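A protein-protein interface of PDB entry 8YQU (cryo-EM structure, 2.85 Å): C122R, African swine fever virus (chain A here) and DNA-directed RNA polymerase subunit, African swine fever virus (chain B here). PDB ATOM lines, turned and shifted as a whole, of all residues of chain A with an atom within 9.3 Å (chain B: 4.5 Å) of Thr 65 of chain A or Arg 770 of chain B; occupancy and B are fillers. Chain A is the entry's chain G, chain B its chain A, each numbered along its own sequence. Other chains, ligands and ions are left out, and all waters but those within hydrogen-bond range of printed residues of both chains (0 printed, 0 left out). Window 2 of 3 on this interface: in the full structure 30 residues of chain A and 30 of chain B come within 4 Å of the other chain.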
ATOM      1  N   PHE A  56     -13.964  27.089  -3.093  1.00  0.00           N
ATOM      2  CA  PHE A  56     -14.936  26.177  -2.502  1.00  0.00           C
ATOM      3  C   PHE A  56     -14.679  24.740  -2.933  1.00  0.00           C
ATOM      4  O   PHE A  56     -14.781  23.816  -2.120  1.00  0.00           O
ATOM      5  CB  PHE A  56     -16.356  26.596  -2.874  1.00  0.00           C
ATOM      6  CG  PHE A  56     -17.396  25.586  -2.492  1.00  0.00           C
ATOM      7  CD1 PHE A  56     -17.786  25.443  -1.172  1.00  0.00           C
ATOM      8  CD2 PHE A  56     -17.976  24.771  -3.450  1.00  0.00           C
ATOM      9  CE1 PHE A  56     -18.738  24.511  -0.814  1.00  0.00           C
ATOM     10  CE2 PHE A  56     -18.929  23.837  -3.097  1.00  0.00           C
ATOM     11  CZ  PHE A  56     -19.309  23.708  -1.777  1.00  0.00           C
ATOM     12  N   ASN A  59     -11.736  23.432  -1.024  1.00  0.00           N
ATOM     13  CA  ASN A  59     -12.027  23.172   0.382  1.00  0.00           C
ATOM     14  C   ASN A  59     -13.088  22.099   0.597  1.00  0.00           C
ATOM     15  O   ASN A  59     -13.261  21.650   1.734  1.00  0.00           O
ATOM     16  CB  ASN A  59     -12.471  24.462   1.072  1.00  0.00           C
ATOM     17  CG  ASN A  59     -11.304  25.321   1.507  1.00  0.00           C
ATOM     18  OD1 ASN A  59     -10.340  24.828   2.089  1.00  0.00           O
ATOM     19  ND2 ASN A  59     -11.387  26.615   1.227  1.00  0.00           N
ATOM     20  N   ALA A  60     -13.800  21.692  -0.451  1.00  0.00           N
ATOM     21  CA  ALA A  60     -14.878  20.717  -0.300  1.00  0.00           C
ATOM     22  C   ALA A  60     -14.472  19.408   0.372  1.00  0.00           C
ATOM     23  O   ALA A  60     -15.234  18.937   1.233  1.00  0.00           O
ATOM     24  CB  ALA A  60     -15.508  20.438  -1.673  1.00  0.00           C
ATOM     25  N   PRO A  61     -13.344  18.766   0.042  1.00  0.00           N
ATOM     26  CA  PRO A  61     -13.021  17.493   0.709  1.00  0.00           C
ATOM     27  C   PRO A  61     -12.853  17.608   2.214  1.00  0.00           C
ATOM     28  O   PRO A  61     -13.033  16.607   2.917  1.00  0.00           O
ATOM     29  CB  PRO A  61     -11.710  17.064   0.036  1.00  0.00           C
ATOM     30  CG  PRO A  61     -11.709  17.762  -1.267  1.00  0.00           C
ATOM     31  CD  PRO A  61     -12.366  19.078  -1.015  1.00  0.00           C
ATOM     32  N   PHE A  62     -12.518  18.789   2.732  1.00  0.00           N
ATOM     33  CA  PHE A  62     -12.311  18.966   4.163  1.00  0.00           C
ATOM     34  C   PHE A  62     -13.536  19.500   4.890  1.00  0.00           C
ATOM     35  O   PHE A  62     -13.594  19.407   6.120  1.00  0.00           O
ATOM     36  CB  PHE A  62     -11.126  19.905   4.413  1.00  0.00           C
ATOM     37  CG  PHE A  62      -9.862  19.469   3.733  1.00  0.00           C
ATOM     38  CD1 PHE A  62      -9.148  18.382   4.203  1.00  0.00           C
ATOM     39  CD2 PHE A  62      -9.392  20.143   2.620  1.00  0.00           C
ATOM     40  CE1 PHE A  62      -7.988  17.977   3.578  1.00  0.00           C
ATOM     41  CE2 PHE A  62      -8.233  19.743   1.990  1.00  0.00           C
ATOM     42  CZ  PHE A  62      -7.529  18.658   2.469  1.00  0.00           C
ATOM     43  N   ASP A  63     -14.501  20.055   4.173  1.00  0.00           N
ATOM     44  CA  ASP A  63     -15.718  20.546   4.802  1.00  0.00           C
ATOM     45  C   ASP A  63     -16.572  19.361   5.236  1.00  0.00           C
ATOM     46  O   ASP A  63     -16.963  18.550   4.387  1.00  0.00           O
ATOM     47  CB  ASP A  63     -16.483  21.438   3.827  1.00  0.00           C
ATOM     48  CG  ASP A  63     -17.655  22.148   4.473  1.00  0.00           C
ATOM     49  OD1 ASP A  63     -17.719  22.194   5.718  1.00  0.00           O
ATOM     50  OD2 ASP A  63     -18.515  22.667   3.730  1.00  0.00           O
ATOM     51  N   PRO A  64     -16.884  19.216   6.527  1.00  0.00           N
ATOM     52  CA  PRO A  64     -17.662  18.051   6.971  1.00  0.00           C
ATOM     53  C   PRO A  64     -19.143  18.126   6.647  1.00  0.00           C
ATOM     54  O   PRO A  64     -19.853  17.135   6.863  1.00  0.00           O
ATOM     55  CB  PRO A  64     -17.435  18.043   8.488  1.00  0.00           C
ATOM     56  CG  PRO A  64     -17.192  19.472   8.828  1.00  0.00           C
ATOM     57  CD  PRO A  64     -16.460  20.064   7.655  1.00  0.00           C
ATOM     58  N   THR A  65     -19.633  19.254   6.139  1.00  0.00           N
ATOM     59  CA  THR A  65     -21.048  19.419   5.838  1.00  0.00           C
ATOM     60  C   THR A  65     -21.396  19.087   4.394  1.00  0.00           C
ATOM     61  O   THR A  65     -22.553  19.254   3.999  1.00  0.00           O
ATOM     62  CB  THR A  65     -21.491  20.850   6.149  1.00  0.00           C
ATOM     63  OG1 THR A  65     -20.983  21.738   5.147  1.00  0.00           O
ATOM     64  CG2 THR A  65     -20.969  21.281   7.505  1.00  0.00           C
ATOM     65  N   ASN A  66     -20.434  18.627   3.600  1.00  0.00           N
ATOM     66  CA  ASN A  66     -20.683  18.282   2.210  1.00  0.00           C
ATOM     67  C   ASN A  66     -21.160  16.840   2.094  1.00  0.00           C
ATOM     68  O   ASN A  66     -20.831  15.986   2.920  1.00  0.00           O
ATOM     69  CB  ASN A  66     -19.424  18.484   1.367  1.00  0.00           C
ATOM     70  CG  ASN A  66     -19.221  19.928   0.965  1.00  0.00           C
ATOM     71  OD1 ASN A  66     -20.167  20.618   0.588  1.00  0.00           O
ATOM     72  ND2 ASN A  66     -17.981  20.394   1.040  1.00  0.00           N
ATOM     73  N   CYS A  67     -21.942  16.577   1.050  1.00  0.00           N
ATOM     74  CA  CYS A  67     -22.493  15.248   0.826  1.00  0.00           C
ATOM     75  C   CYS A  67     -21.415  14.308   0.303  1.00  0.00           C
ATOM     76  O   CYS A  67     -20.707  14.633  -0.655  1.00  0.00           O
ATOM     77  CB  CYS A  67     -23.658  15.313  -0.158  1.00  0.00           C
ATOM     78  SG  CYS A  67     -24.477  13.731  -0.452  1.00  0.00           S
ATOM     79  N   GLN A  68     -21.290  13.148   0.935  1.00  0.00           N
ATOM     80  CA  GLN A  68     -20.351  12.127   0.499  1.00  0.00           C
ATOM     81  C   GLN A  68     -21.059  11.093  -0.370  1.00  0.00           C
ATOM     82  O   GLN A  68     -22.289  11.011  -0.406  1.00  0.00           O
ATOM     83  CB  GLN A  68     -19.696  11.447   1.700  1.00  0.00           C
ATOM     84  CG  GLN A  68     -19.126  12.410   2.726  1.00  0.00           C
ATOM     85  CD  GLN A  68     -17.833  13.048   2.273  1.00  0.00           C
ATOM     86  OE1 GLN A  68     -16.933  12.371   1.778  1.00  0.00           O
ATOM     87  NE2 GLN A  68     -17.730  14.361   2.441  1.00  0.00           N
ATOM     88  N   THR A  82     -16.362  12.980  -2.169  1.00  0.00           N
ATOM     89  CA  THR A  82     -17.222  14.107  -1.835  1.00  0.00           C
ATOM     90  C   THR A  82     -17.907  14.591  -3.107  1.00  0.00           C
ATOM     91  O   THR A  82     -17.236  14.953  -4.077  1.00  0.00           O
ATOM     92  CB  THR A  82     -16.424  15.239  -1.191  1.00  0.00           C
ATOM     93  OG1 THR A  82     -15.787  14.759   0.000  1.00  0.00           O
ATOM     94  CG2 THR A  82     -17.339  16.398  -0.839  1.00  0.00           C
ATOM     95  N   GLN A  83     -19.235  14.602  -3.097  1.00  0.00           N
ATOM     96  CA  GLN A  83     -20.035  14.937  -4.267  1.00  0.00           C
ATOM     97  C   GLN A  83     -20.609  16.337  -4.097  1.00  0.00           C
ATOM     98  O   GLN A  83     -21.250  16.628  -3.082  1.00  0.00           O
ATOM     99  CB  GLN A  83     -21.155  13.916  -4.465  1.00  0.00           C
ATOM    100  CG  GLN A  83     -22.188  14.308  -5.504  1.00  0.00           C
ATOM    101  CD  GLN A  83     -23.472  14.819  -4.881  1.00  0.00           C
ATOM    102  OE1 GLN A  83     -23.790  14.496  -3.737  1.00  0.00           O
ATOM    103  NE2 GLN A  83     -24.217  15.620  -5.631  1.00  0.00           N
ATOM    104  N   ILE A  84     -20.377  17.199  -5.084  1.00  0.00           N
ATOM    105  CA  ILE A  84     -20.929  18.547  -5.077  1.00  0.00           C
ATOM    106  C   ILE A  84     -21.687  18.772  -6.376  1.00  0.00           C
ATOM    107  O   ILE A  84     -21.362  18.196  -7.420  1.00  0.00           O
ATOM    108  CB  ILE A  84     -19.841  19.625  -4.878  1.00  0.00           C
ATOM    109  CG1 ILE A  84     -18.837  19.600  -6.028  1.00  0.00           C
ATOM    110  CG2 ILE A  84     -19.130  19.430  -3.550  1.00  0.00           C
ATOM    111  CD1 ILE A  84     -17.810  20.703  -5.953  1.00  0.00           C
ATOM    112  N   PRO B 764     -33.168  25.702  -0.477  1.00  0.00           N
ATOM    113  CA  PRO B 764     -32.119  25.781   0.551  1.00  0.00           C
ATOM    114  C   PRO B 764     -31.782  27.208   0.960  1.00  0.00           C
ATOM    115  O   PRO B 764     -31.100  27.921   0.217  1.00  0.00           O
ATOM    116  CB  PRO B 764     -30.919  25.104  -0.121  1.00  0.00           C
ATOM    117  CG  PRO B 764     -31.170  25.248  -1.581  1.00  0.00           C
ATOM    118  CD  PRO B 764     -32.652  25.218  -1.768  1.00  0.00           C
ATOM    119  N   GLN B 765     -32.236  27.638   2.138  1.00  0.00           N
ATOM    120  CA  GLN B 765     -31.847  28.929   2.689  1.00  0.00           C
ATOM    121  C   GLN B 765     -30.805  28.817   3.792  1.00  0.00           C
ATOM    122  O   GLN B 765     -30.456  29.835   4.398  1.00  0.00           O
ATOM    123  CB  GLN B 765     -33.062  29.695   3.231  1.00  0.00           C
ATOM    124  CG  GLN B 765     -34.060  30.165   2.184  1.00  0.00           C
ATOM    125  CD  GLN B 765     -35.062  29.098   1.810  1.00  0.00           C
ATOM    126  OE1 GLN B 765     -35.242  28.120   2.535  1.00  0.00           O
ATOM    127  NE2 GLN B 765     -35.730  29.283   0.677  1.00  0.00           N
ATOM    128  N   PHE B 766     -30.303  27.619   4.076  1.00  0.00           N
ATOM    129  CA  PHE B 766     -29.334  27.404   5.147  1.00  0.00           C
ATOM    130  C   PHE B 766     -27.955  27.199   4.523  1.00  0.00           C
ATOM    131  O   PHE B 766     -27.508  26.073   4.307  1.00  0.00           O
ATOM    132  CB  PHE B 766     -29.752  26.213   6.027  1.00  0.00           C
ATOM    133  CG  PHE B 766     -28.889  26.019   7.241  1.00  0.00           C
ATOM    134  CD1 PHE B 766     -29.135  26.730   8.401  1.00  0.00           C
ATOM    135  CD2 PHE B 766     -27.841  25.117   7.225  1.00  0.00           C
ATOM    136  CE1 PHE B 766     -28.347  26.551   9.519  1.00  0.00           C
ATOM    137  CE2 PHE B 766     -27.049  24.935   8.339  1.00  0.00           C
ATOM    138  CZ  PHE B 766     -27.303  25.652   9.487  1.00  0.00           C
ATOM    139  N   SER B 767     -27.281  28.311   4.230  1.00  0.00           N
ATOM    140  CA  SER B 767     -25.855  28.334   3.902  1.00  0.00           C
ATOM    141  C   SER B 767     -25.533  27.494   2.659  1.00  0.00           C
ATOM    142  O   SER B 767     -24.826  26.485   2.716  1.00  0.00           O
ATOM    143  CB  SER B 767     -25.022  27.868   5.101  1.00  0.00           C
ATOM    144  OG  SER B 767     -24.966  26.454   5.162  1.00  0.00           O
ATOM    145  N   PHE B 768     -26.072  27.950   1.526  1.00  0.00           N
ATOM    146  CA  PHE B 768     -25.593  27.560   0.195  1.00  0.00           C
ATOM    147  C   PHE B 768     -25.673  26.043  -0.019  1.00  0.00           C
ATOM    148  O   PHE B 768     -24.671  25.327  -0.057  1.00  0.00           O
ATOM    149  CB  PHE B 768     -24.168  28.080  -0.040  1.00  0.00           C
ATOM    150  CG  PHE B 768     -23.556  27.608  -1.331  1.00  0.00           C
ATOM    151  CD1 PHE B 768     -24.214  27.796  -2.535  1.00  0.00           C
ATOM    152  CD2 PHE B 768     -22.329  26.966  -1.337  1.00  0.00           C
ATOM    153  CE1 PHE B 768     -23.657  27.357  -3.719  1.00  0.00           C
ATOM    154  CE2 PHE B 768     -21.768  26.527  -2.519  1.00  0.00           C
ATOM    155  CZ  PHE B 768     -22.433  26.722  -3.711  1.00  0.00           C
ATOM    156  N   GLY B 769     -26.908  25.564  -0.117  1.00  0.00           N
ATOM    157  CA  GLY B 769     -27.168  24.206  -0.551  1.00  0.00           C
ATOM    158  C   GLY B 769     -27.726  23.293   0.512  1.00  0.00           C
ATOM    159  O   GLY B 769     -28.149  22.177   0.184  1.00  0.00           O
ATOM    160  N   ARG B 770     -27.744  23.719   1.769  1.00  0.00           N
ATOM    161  CA  ARG B 770     -28.339  22.947   2.847  1.00  0.00           C
ATOM    162  C   ARG B 770     -29.719  23.508   3.149  1.00  0.00           C
ATOM    163  O   ARG B 770     -29.875  24.721   3.318  1.00  0.00           O
ATOM    164  CB  ARG B 770     -27.464  22.990   4.100  1.00  0.00           C
ATOM    165  CG  ARG B 770     -25.982  22.834   3.832  1.00  0.00           C
ATOM    166  CD  ARG B 770     -25.198  22.838   5.128  1.00  0.00           C
ATOM    167  NE  ARG B 770     -25.492  21.669   5.946  1.00  0.00           N
ATOM    168  CZ  ARG B 770     -25.239  21.582   7.244  1.00  0.00           C
ATOM    169  NH1 ARG B 770     -24.680  22.580   7.907  1.00  0.00           N
ATOM    170  NH2 ARG B 770     -25.555  20.466   7.894  1.00  0.00           N
ATOM    171  N   THR B 771     -30.721  22.632   3.183  1.00  0.00           N
ATOM    172  CA  THR B 771     -32.055  23.062   3.581  1.00  0.00           C
ATOM    173  C   THR B 771     -32.171  23.227   5.090  1.00  0.00           C
ATOM    174  O   THR B 771     -32.873  24.130   5.558  1.00  0.00           O
ATOM    175  CB  THR B 771     -33.101  22.070   3.075  1.00  0.00           C
ATOM    176  OG1 THR B 771     -32.748  20.748   3.499  1.00  0.00           O
ATOM    177  CG2 THR B 771     -33.168  22.106   1.559  1.00  0.00           C
ATOM    178  N   LEU B 772     -31.493  22.376   5.857  1.00  0.00           N
ATOM    179  CA  LEU B 772     -31.469  22.468   7.309  1.00  0.00           C
ATOM    180  C   LEU B 772     -30.094  22.048   7.804  1.00  0.00           C
ATOM    181  O   LEU B 772     -29.244  21.592   7.037  1.00  0.00           O
ATOM    182  CB  LEU B 772     -32.554  21.596   7.955  1.00  0.00           C
ATOM    183  CG  LEU B 772     -33.995  22.106   7.933  1.00  0.00           C
ATOM    184  CD1 LEU B 772     -34.920  21.082   8.564  1.00  0.00           C
ATOM    185  CD2 LEU B 772     -34.101  23.438   8.651  1.00  0.00           C
ATOM    186  N   VAL B 773     -29.880  22.205   9.113  1.00  0.00           N
ATOM    187  CA  VAL B 773     -28.621  21.792   9.715  1.00  0.00           C
ATOM    188  C   VAL B 773     -28.519  20.274   9.799  1.00  0.00           C
ATOM    189  O   VAL B 773     -27.421  19.735   9.979  1.00  0.00           O
ATOM    190  CB  VAL B 773     -28.463  22.443  11.104  1.00  0.00           C
ATOM    191  CG1 VAL B 773     -29.441  21.836  12.095  1.00  0.00           C
ATOM    192  CG2 VAL B 773     -27.029  22.329  11.604  1.00  0.00           C
ATOM    193  N   TYR B 775     -29.138  18.133   7.365  1.00  0.00           N
ATOM    194  CA  TYR B 775     -28.814  17.520   6.091  1.00  0.00           C
ATOM    195  C   TYR B 775     -27.556  18.142   5.498  1.00  0.00           C
ATOM    196  O   TYR B 775     -27.311  19.341   5.667  1.00  0.00           O
ATOM    197  CB  TYR B 775     -29.976  17.663   5.102  1.00  0.00           C
ATOM    198  CG  TYR B 775     -31.256  17.030   5.590  1.00  0.00           C
ATOM    199  CD1 TYR B 775     -31.390  15.650   5.644  1.00  0.00           C
ATOM    200  CD2 TYR B 775     -32.328  17.809   6.004  1.00  0.00           C
ATOM    201  CE1 TYR B 775     -32.552  15.063   6.092  1.00  0.00           C
ATOM    202  CE2 TYR B 775     -33.497  17.228   6.455  1.00  0.00           C
ATOM    203  CZ  TYR B 775     -33.602  15.855   6.495  1.00  0.00           C
ATOM    204  OH  TYR B 775     -34.760  15.263   6.939  1.00  0.00           O
ATOM    205  N   PRO B 776     -26.742  17.356   4.802  1.00  0.00           N
ATOM    206  CA  PRO B 776     -25.481  17.872   4.268  1.00  0.00           C
ATOM    207  C   PRO B 776     -25.706  18.763   3.054  1.00  0.00           C
ATOM    208  O   PRO B 776     -26.793  18.835   2.482  1.00  0.00           O
ATOM    209  CB  PRO B 776     -24.719  16.600   3.887  1.00  0.00           C
ATOM    210  CG  PRO B 776     -25.787  15.626   3.561  1.00  0.00           C
ATOM    211  CD  PRO B 776     -26.918  15.924   4.506  1.00  0.00           C
ATOM    212  N   ARG B 777     -24.636  19.456   2.673  1.00  0.00           N
ATOM    213  CA  ARG B 777     -24.683  20.336   1.515  1.00  0.00           C
ATOM    214  C   ARG B 777     -24.826  19.520   0.236  1.00  0.00           C
ATOM    215  O   ARG B 777     -24.207  18.464   0.082  1.00  0.00           O
ATOM    216  CB  ARG B 777     -23.422  21.195   1.460  1.00  0.00           C
ATOM    217  CG  ARG B 777     -23.469  22.311   0.438  1.00  0.00           C
ATOM    218  CD  ARG B 777     -22.246  23.202   0.554  1.00  0.00           C
ATOM    219  NE  ARG B 777     -22.383  24.170   1.635  1.00  0.00           N
ATOM    220  CZ  ARG B 777     -21.580  24.233   2.688  1.00  0.00           C
ATOM    221  NH1 ARG B 777     -20.569  23.395   2.838  1.00  0.00           N
ATOM    222  NH2 ARG B 777     -21.799  25.162   3.614  1.00  0.00           N
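Of the 14 printed residues of chain A, 5 touch a printed residue of chain B. Of the 13 printed residues of chain B, 4 touch a printed residue of chain A. Hydrophobic or aromatic side chains of chain B within 4 Å of the printed part of chain A: Phe 768 and Pro 776. Among the printed residues, 10 pairs touch across the chains. Among the printed residues, Asp or Glu carboxylates within 4 Å of a Lys or Arg side-chain nitrogen of the other chain: Asp 63 of chain A with Arg 777 of chain B (2.4 Å).
Among the printed residues, merely in contact across the chains: Phe 56 of chain A with Phe 768 of chain B (3.8 Å), Phe 56 of chain A with Arg 777 of chain B (3.8 Å), Thr 65 of chain A with Arg 770 of chain B (3.95 Å), Thr 65 of chain A with Pro 776 of chain B (3.2 Å), Asn 66 of chain A with Pro 776 of chain B (3.99 Å), Asn 66 of chain A with Arg 777 of chain B (3.3 Å) and Cys 67 of chain A with Pro 776 of chain B (3.97 Å).
The backbone carbonyl oxygen (O) of Ser 767 of chain B sits at hydrogen-bond distance from the guanidinium group (NH2) of Arg 777 of chain B (3.4 Å). NE of Arg 770 of chain B is in hydrogen-bond range of O of Tyr 775 of chain B, 3.0 Å away. O of Cys 67 of chain A is in hydrogen-bond range of N of Gln 83 of chain A (2.9 Å). O of Ala 60 of chain A sits at hydrogen-bond distance from ND2 of Asn 66 of chain A (3.1 Å). The side-chain hydroxyl (OG1) of Thr 65 of chain A lies within hydrogen-bond range of the side-chain carboxylate (OD2) of Asp 63 of chain A (3.0 Å). O of Phe 768 of chain B is in hydrogen-bond range of NE of Arg 777 of chain B (3.1 Å).
The backbone carbonyl oxygen of Arg 777 of chain B is in hydrogen-bond range of the backbone NH of Cys 67 of chain A (3.1 Å). NH1 of Arg 777 of chain B sits close to OD2 of Asp 63 of chain A (2.4 Å). N of Arg 777 of chain B is in hydrogen-bond range of O of Thr 65 of chain A, at 2.5 Å.
Of the printed residues of chain B, Asp 63 of chain A touches Arg 777 (2.4 Å). Thr 65 of chain A touches just these residues of chain B: Arg 770 (3.95 Å), Pro 776 (3.2 Å) and Arg 777 (2.5 Å). Gln 68 of chain A touches none of the printed residues of chain B. Printed residues of chain A within 4 Å of Phe 768 of chain B: Phe 56. Of chain A, only Thr 65 (3.95 Å) comes within 4 Å of Arg 770 of chain B. No residue of chain A comes within 4 Å of Thr 771 of chain B. Tyr 775 of chain B touches none of the printed residues of chain A. Of chain A, only Phe 56 (3.8 Å), Asp 63 (2.4 Å), Thr 65 (2.5 Å), Asn 66 (3.3 Å) and Cys 67 (3.1 Å) come within 4 Å of Arg 777 of chain B. The nearest residue of chain A that does not touch Arg 770 of chain B is Asn 66 of chain A (6.4 Å). The nearest printed residue of chain A that does not touch Pro 776 of chain B is Gln 68 of chain A (5.7 Å).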
